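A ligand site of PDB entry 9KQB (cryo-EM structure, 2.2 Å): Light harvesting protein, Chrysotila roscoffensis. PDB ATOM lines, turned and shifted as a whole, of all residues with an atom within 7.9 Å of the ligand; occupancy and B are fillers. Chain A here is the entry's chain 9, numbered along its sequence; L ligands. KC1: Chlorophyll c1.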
ATOM      1  N   MET A  86      11.043  10.207  14.827  1.00  0.00           N
ATOM      2  CA  MET A  86      10.004   9.479  14.109  1.00  0.00           C
ATOM      3  C   MET A  86       9.887   9.956  12.669  1.00  0.00           C
ATOM      4  O   MET A  86       9.977   9.158  11.733  1.00  0.00           O
ATOM      5  CB  MET A  86       8.638   9.643  14.775  1.00  0.00           C
ATOM      6  CG  MET A  86       8.545   9.488  16.275  1.00  0.00           C
ATOM      7  SD  MET A  86       7.809   7.916  16.777  1.00  0.00           S
ATOM      8  CE  MET A  86       7.369   8.297  18.473  1.00  0.00           C
ATOM      9  N   THR A  89      12.444   8.835  10.325  1.00  0.00           N
ATOM     10  CA  THR A  89      12.346   7.438   9.903  1.00  0.00           C
ATOM     11  C   THR A  89      11.321   7.275   8.785  1.00  0.00           C
ATOM     12  O   THR A  89      11.562   6.543   7.812  1.00  0.00           O
ATOM     13  CB  THR A  89      11.987   6.526  11.084  1.00  0.00           C
ATOM     14  OG1 THR A  89      10.830   7.038  11.759  1.00  0.00           O
ATOM     15  CG2 THR A  89      13.140   6.396  12.057  1.00  0.00           C
ATOM     16  N   LEU A  90      10.167   7.939   8.915  1.00  0.00           N
ATOM     17  CA  LEU A  90       9.155   7.892   7.866  1.00  0.00           C
ATOM     18  C   LEU A  90       9.629   8.572   6.584  1.00  0.00           C
ATOM     19  O   LEU A  90       9.155   8.228   5.494  1.00  0.00           O
ATOM     20  CB  LEU A  90       7.817   8.489   8.317  1.00  0.00           C
ATOM     21  CG  LEU A  90       6.868   7.829   9.348  1.00  0.00           C
ATOM     22  CD1 LEU A  90       6.256   6.561   8.772  1.00  0.00           C
ATOM     23  CD2 LEU A  90       7.432   7.488  10.693  1.00  0.00           C
ATOM     24  N   PHE A  93      11.920   6.077   4.853  1.00  0.00           N
ATOM     25  CA  PHE A  93      11.195   4.878   4.459  1.00  0.00           C
ATOM     26  C   PHE A  93      10.337   5.125   3.226  1.00  0.00           C
ATOM     27  O   PHE A  93      10.212   4.244   2.370  1.00  0.00           O
ATOM     28  CB  PHE A  93      10.333   4.384   5.618  1.00  0.00           C
ATOM     29  CG  PHE A  93      11.084   3.559   6.623  1.00  0.00           C
ATOM     30  CD1 PHE A  93      12.254   2.907   6.269  1.00  0.00           C
ATOM     31  CD2 PHE A  93      10.620   3.425   7.921  1.00  0.00           C
ATOM     32  CE1 PHE A  93      12.958   2.153   7.196  1.00  0.00           C
ATOM     33  CE2 PHE A  93      11.310   2.675   8.850  1.00  0.00           C
ATOM     34  CZ  PHE A  93      12.475   2.035   8.491  1.00  0.00           C
ATOM     35  N   VAL A 174      -7.399   5.175  27.186  1.00  0.00           N
ATOM     36  CA  VAL A 174      -6.861   4.992  25.842  1.00  0.00           C
ATOM     37  C   VAL A 174      -5.686   5.929  25.600  1.00  0.00           C
ATOM     38  O   VAL A 174      -4.687   5.550  24.971  1.00  0.00           O
ATOM     39  CB  VAL A 174      -7.968   5.189  24.784  1.00  0.00           C
ATOM     40  CG1 VAL A 174      -8.775   3.912  24.624  1.00  0.00           C
ATOM     41  CG2 VAL A 174      -8.894   6.333  25.178  1.00  0.00           C
ATOM     42  N   LYS A 175      -5.793   7.168  26.092  1.00  0.00           N
ATOM     43  CA  LYS A 175      -4.756   8.156  25.797  1.00  0.00           C
ATOM     44  C   LYS A 175      -3.505   7.946  26.638  1.00  0.00           C
ATOM     45  O   LYS A 175      -2.395   8.251  26.191  1.00  0.00           O
ATOM     46  CB  LYS A 175      -5.313   9.579  25.987  1.00  0.00           C
ATOM     47  CG  LYS A 175      -5.641   9.970  27.417  1.00  0.00           C
ATOM     48  CD  LYS A 175      -5.579  11.464  27.618  1.00  0.00           C
ATOM     49  CE  LYS A 175      -4.185  11.911  28.029  1.00  0.00           C
ATOM     50  NZ  LYS A 175      -4.191  13.234  28.717  1.00  0.00           N
ATOM     51  N   TYR A 177      -2.190   5.109  27.551  1.00  0.00           N
ATOM     52  CA  TYR A 177      -1.399   4.047  26.942  1.00  0.00           C
ATOM     53  C   TYR A 177      -0.848   4.474  25.585  1.00  0.00           C
ATOM     54  O   TYR A 177       0.229   4.005  25.193  1.00  0.00           O
ATOM     55  CB  TYR A 177      -2.253   2.782  26.798  1.00  0.00           C
ATOM     56  CG  TYR A 177      -1.464   1.552  26.379  1.00  0.00           C
ATOM     57  CD1 TYR A 177      -0.193   1.309  26.883  1.00  0.00           C
ATOM     58  CD2 TYR A 177      -2.013   0.632  25.487  1.00  0.00           C
ATOM     59  CE1 TYR A 177       0.516   0.181  26.494  1.00  0.00           C
ATOM     60  CE2 TYR A 177      -1.312  -0.494  25.093  1.00  0.00           C
ATOM     61  CZ  TYR A 177      -0.041  -0.716  25.606  1.00  0.00           C
ATOM     62  OH  TYR A 177       0.657  -1.831  25.220  1.00  0.00           O
ATOM     63  N   LYS A 178      -1.560   5.359  24.883  1.00  0.00           N
ATOM     64  CA  LYS A 178      -1.107   5.789  23.555  1.00  0.00           C
ATOM     65  C   LYS A 178       0.152   6.648  23.651  1.00  0.00           C
ATOM     66  O   LYS A 178       1.018   6.581  22.782  1.00  0.00           O
ATOM     67  CB  LYS A 178      -2.230   6.546  22.849  1.00  0.00           C
ATOM     68  CG  LYS A 178      -3.132   5.655  22.013  1.00  0.00           C
ATOM     69  CD  LYS A 178      -4.326   6.419  21.477  1.00  0.00           C
ATOM     70  CE  LYS A 178      -5.429   5.472  21.009  1.00  0.00           C
ATOM     71  NZ  LYS A 178      -5.046   4.720  19.783  1.00  0.00           N
ATOM     72  N   LEU A 179       0.261   7.478  24.698  1.00  0.00           N
ATOM     73  CA  LEU A 179       1.484   8.246  24.891  1.00  0.00           C
ATOM     74  C   LEU A 179       2.640   7.335  25.294  1.00  0.00           C
ATOM     75  O   LEU A 179       3.792   7.582  24.921  1.00  0.00           O
ATOM     76  CB  LEU A 179       1.267   9.340  25.936  1.00  0.00           C
ATOM     77  CG  LEU A 179       0.672   9.017  27.312  1.00  0.00           C
ATOM     78  CD1 LEU A 179       1.750   8.757  28.345  1.00  0.00           C
ATOM     79  CD2 LEU A 179      -0.222  10.159  27.765  1.00  0.00           C
ATOM     80  N   ASN A 180       2.349   6.279  26.061  1.00  0.00           N
ATOM     81  CA  ASN A 180       3.370   5.296  26.390  1.00  0.00           C
ATOM     82  C   ASN A 180       3.788   4.514  25.155  1.00  0.00           C
ATOM     83  O   ASN A 180       4.953   4.129  25.011  1.00  0.00           O
ATOM     84  CB  ASN A 180       2.863   4.358  27.482  1.00  0.00           C
ATOM     85  CG  ASN A 180       3.014   4.944  28.870  1.00  0.00           C
ATOM     86  OD1 ASN A 180       4.123   5.194  29.338  1.00  0.00           O
ATOM     87  ND2 ASN A 180       1.888   5.178  29.537  1.00  0.00           N
ATOM     88  N   ILE A 181       2.841   4.242  24.251  1.00  0.00           N
ATOM     89  CA  ILE A 181       3.175   3.664  22.957  1.00  0.00           C
ATOM     90  C   ILE A 181       4.022   4.636  22.149  1.00  0.00           C
ATOM     91  O   ILE A 181       5.018   4.247  21.520  1.00  0.00           O
ATOM     92  CB  ILE A 181       1.882   3.266  22.206  1.00  0.00           C
ATOM     93  CG1 ILE A 181       1.267   2.007  22.818  1.00  0.00           C
ATOM     94  CG2 ILE A 181       2.142   3.074  20.729  1.00  0.00           C
ATOM     95  CD1 ILE A 181      -0.130   1.711  22.337  1.00  0.00           C
ATOM     96  N   GLU A 182       3.644   5.919  22.176  1.00  0.00           N
ATOM     97  CA  GLU A 182       4.414   6.945  21.479  1.00  0.00           C
ATOM     98  C   GLU A 182       5.807   7.089  22.072  1.00  0.00           C
ATOM     99  O   GLU A 182       6.794   7.229  21.338  1.00  0.00           O
ATOM    100  CB  GLU A 182       3.654   8.276  21.538  1.00  0.00           C
ATOM    101  CG  GLU A 182       4.437   9.491  21.061  1.00  0.00           C
ATOM    102  CD  GLU A 182       3.685  10.790  21.253  1.00  0.00           C
ATOM    103  OE1 GLU A 182       2.983  10.926  22.278  1.00  0.00           O
ATOM    104  OE2 GLU A 182       3.788  11.675  20.387  1.00  0.00           O
ATOM    105  N   ASN A 184       7.472   4.738  23.714  1.00  0.00           N
ATOM    106  CA  ASN A 184       8.211   3.526  23.369  1.00  0.00           C
ATOM    107  C   ASN A 184       8.601   3.516  21.901  1.00  0.00           C
ATOM    108  O   ASN A 184       9.709   3.089  21.538  1.00  0.00           O
ATOM    109  CB  ASN A 184       7.402   2.285  23.732  1.00  0.00           C
ATOM    110  CG  ASN A 184       8.123   0.995  23.395  1.00  0.00           C
ATOM    111  OD1 ASN A 184       9.355   0.917  23.484  1.00  0.00           O
ATOM    112  ND2 ASN A 184       7.376  -0.021  22.989  1.00  0.00           N
ATOM    113  N   ASN A 185       7.710   3.975  21.012  1.00  0.00           N
ATOM    114  CA  ASN A 185       8.052   4.006  19.591  1.00  0.00           C
ATOM    115  C   ASN A 185       9.033   5.123  19.290  1.00  0.00           C
ATOM    116  O   ASN A 185       9.750   5.086  18.288  1.00  0.00           O
ATOM    117  CB  ASN A 185       6.805   4.114  18.702  1.00  0.00           C
ATOM    118  CG  ASN A 185       5.916   2.837  18.706  1.00  0.00           C
ATOM    119  OD1 ASN A 185       5.546   2.328  17.647  1.00  0.00           O
ATOM    120  ND2 ASN A 185       5.579   2.355  19.889  1.00  0.00           N
ATOM    121  N   GLY A 186       9.056   6.156  20.143  1.00  0.00           N
ATOM    122  CA  GLY A 186      10.047   7.209  19.991  1.00  0.00           C
ATOM    123  C   GLY A 186      11.441   6.743  20.387  1.00  0.00           C
ATOM    124  O   GLY A 186      12.436   7.202  19.817  1.00  0.00           O
ATOM    125  N   ARG A 187      11.528   5.850  21.375  1.00  0.00           N
ATOM    126  CA  ARG A 187      12.814   5.318  21.801  1.00  0.00           C
ATOM    127  C   ARG A 187      13.427   4.442  20.714  1.00  0.00           C
ATOM    128  O   ARG A 187      14.651   4.450  20.505  1.00  0.00           O
ATOM    129  CB  ARG A 187      12.659   4.540  23.097  1.00  0.00           C
ATOM    130  CG  ARG A 187      12.473   5.426  24.324  1.00  0.00           C
ATOM    131  CD  ARG A 187      11.763   4.686  25.446  1.00  0.00           C
ATOM    132  NE  ARG A 187      11.378   5.595  26.518  1.00  0.00           N
ATOM    133  CZ  ARG A 187      10.967   5.214  27.723  1.00  0.00           C
ATOM    134  NH1 ARG A 187      10.887   3.925  28.051  1.00  0.00           N
ATOM    135  NH2 ARG A 187      10.625   6.124  28.616  1.00  0.00           N
ATOM    136  N   ALA A 188      12.589   3.681  20.006  1.00  0.00           N
ATOM    137  CA  ALA A 188      13.087   2.846  18.918  1.00  0.00           C
ATOM    138  C   ALA A 188      13.481   3.688  17.710  1.00  0.00           C
ATOM    139  O   ALA A 188      14.479   3.396  17.033  1.00  0.00           O
ATOM    140  CB  ALA A 188      12.035   1.818  18.521  1.00  0.00           C
ATOM    141  N   ALA A 189      12.705   4.738  17.409  1.00  0.00           N
ATOM    142  CA  ALA A 189      12.995   5.594  16.261  1.00  0.00           C
ATOM    143  C   ALA A 189      14.260   6.402  16.466  1.00  0.00           C
ATOM    144  O   ALA A 189      14.966   6.728  15.499  1.00  0.00           O
ATOM    145  CB  ALA A 189      11.804   6.515  15.979  1.00  0.00           C
HETATM  146  NB  KC1 L   1       5.504   1.581  14.758  1.00  0.00           N
HETATM  147  ND  KC1 L   1       4.430  -0.088  18.312  1.00  0.00           N
HETATM  148  C1A KC1 L   1       1.918   1.339  16.944  1.00  0.00           C
HETATM  149  C1B KC1 L   1       4.790   2.360  13.944  1.00  0.00           C
HETATM  150  C1C KC1 L   1       7.790   0.056  16.162  1.00  0.00           C
HETATM  151  C1D KC1 L   1       5.029  -0.913  19.333  1.00  0.00           C
HETATM  152  C2A KC1 L   1       0.680   2.030  16.435  1.00  0.00           C
HETATM  153  C2B KC1 L   1       5.522   2.881  12.764  1.00  0.00           C
HETATM  154  C2C KC1 L   1       9.013  -0.658  16.614  1.00  0.00           C
HETATM  155  C2D KC1 L   1       4.100  -1.453  20.352  1.00  0.00           C
HETATM  156  C3A KC1 L   1       1.181   2.673  15.153  1.00  0.00           C
HETATM  157  C3B KC1 L   1       6.875   2.295  12.973  1.00  0.00           C
HETATM  158  C3C KC1 L   1       8.612  -1.215  17.920  1.00  0.00           C
HETATM  159  C3D KC1 L   1       2.821  -0.877  19.865  1.00  0.00           C
HETATM  160  C4A KC1 L   1       2.610   2.233  15.201  1.00  0.00           C
HETATM  161  C4B KC1 L   1       6.726   1.507  14.238  1.00  0.00           C
HETATM  162  C4C KC1 L   1       7.199  -0.751  18.051  1.00  0.00           C
HETATM  163  C4D KC1 L   1       3.112  -0.136  18.717  1.00  0.00           C
HETATM  164  CAA KC1 L   1       0.212   3.160  17.349  1.00  0.00           C
HETATM  165  CAB KC1 L   1       8.082   2.447  12.121  1.00  0.00           C
HETATM  166  CAC KC1 L   1       9.427  -2.053  18.885  1.00  0.00           C
HETATM  167  CAD KC1 L   1       1.354  -0.760  20.109  1.00  0.00           C
HETATM  168  CBA KC1 L   1      -1.316   3.238  17.347  1.00  0.00           C
HETATM  169  CBB KC1 L   1       8.748   1.408  11.655  1.00  0.00           C
HETATM  170  CBC KC1 L   1      10.016  -1.079  19.885  1.00  0.00           C
HETATM  171  CBD KC1 L   1       0.750   0.070  19.047  1.00  0.00           C
HETATM  172  CED KC1 L   1      -2.298  -1.363  17.159  1.00  0.00           C
HETATM  173  CGA KC1 L   1      -1.819   3.334  18.762  1.00  0.00           C
HETATM  174  CGD KC1 L   1      -0.084  -0.838  18.199  1.00  0.00           C
HETATM  175  CHA KC1 L   1       1.896   0.508  18.193  1.00  0.00           C
HETATM  176  CHB KC1 L   1       3.367   2.652  14.187  1.00  0.00           C
HETATM  177  CHC KC1 L   1       7.827   0.752  14.854  1.00  0.00           C
HETATM  178  CHD KC1 L   1       6.477  -1.154  19.286  1.00  0.00           C
HETATM  179  CMA KC1 L   1       0.495   2.052  13.933  1.00  0.00           C
HETATM  180  CMB KC1 L   1       5.027   3.769  11.649  1.00  0.00           C
HETATM  181  CMC KC1 L   1      10.337  -0.787  15.914  1.00  0.00           C
HETATM  182  CMD KC1 L   1       4.211  -2.328  21.576  1.00  0.00           C
HETATM  183  NA  KC1 L   1       2.974   1.470  16.234  1.00  0.00           N
HETATM  184  NC  KC1 L   1       6.747  -0.005  17.008  1.00  0.00           N
HETATM  185  O1A KC1 L   1      -2.956   2.987  19.036  1.00  0.00           O
HETATM  186  O1D KC1 L   1       0.433  -1.696  17.509  1.00  0.00           O
HETATM  187  O2A KC1 L   1      -0.965   3.860  19.817  1.00  0.00           O
HETATM  188  O2D KC1 L   1      -1.534  -0.696  18.171  1.00  0.00           O
HETATM  189  OBD KC1 L   1       0.728  -1.325  21.074  1.00  0.00           O
HETATM  190 MG   KC1 L   1       4.863   0.624  16.458  1.00  0.00          MG
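OD1 of Asn 185 is bound to MG of the ligand (2.2 Å).
NZ of Lys 178 lies within salt-bridge range of O1A of the ligand (2.8 Å).
The backbone carbonyl oxygen (O) of Ile 181 sits at hydrogen-bond distance from the side-chain amide nitrogen (ND2) of Asn 185, 2.6 Å away.
Residues that only touch the ligand: Ile 181 (3.3 Å), Asn 184 (3.98 Å) and Ala 188 (3.8 Å).
Hydrophobic or aromatic side chains that line the ligand: Ile 181 and Ala 188.
Within 4 Å of the ligand: Lys 178, Ile 181, Asn 184, Asn 185 and Ala 188.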
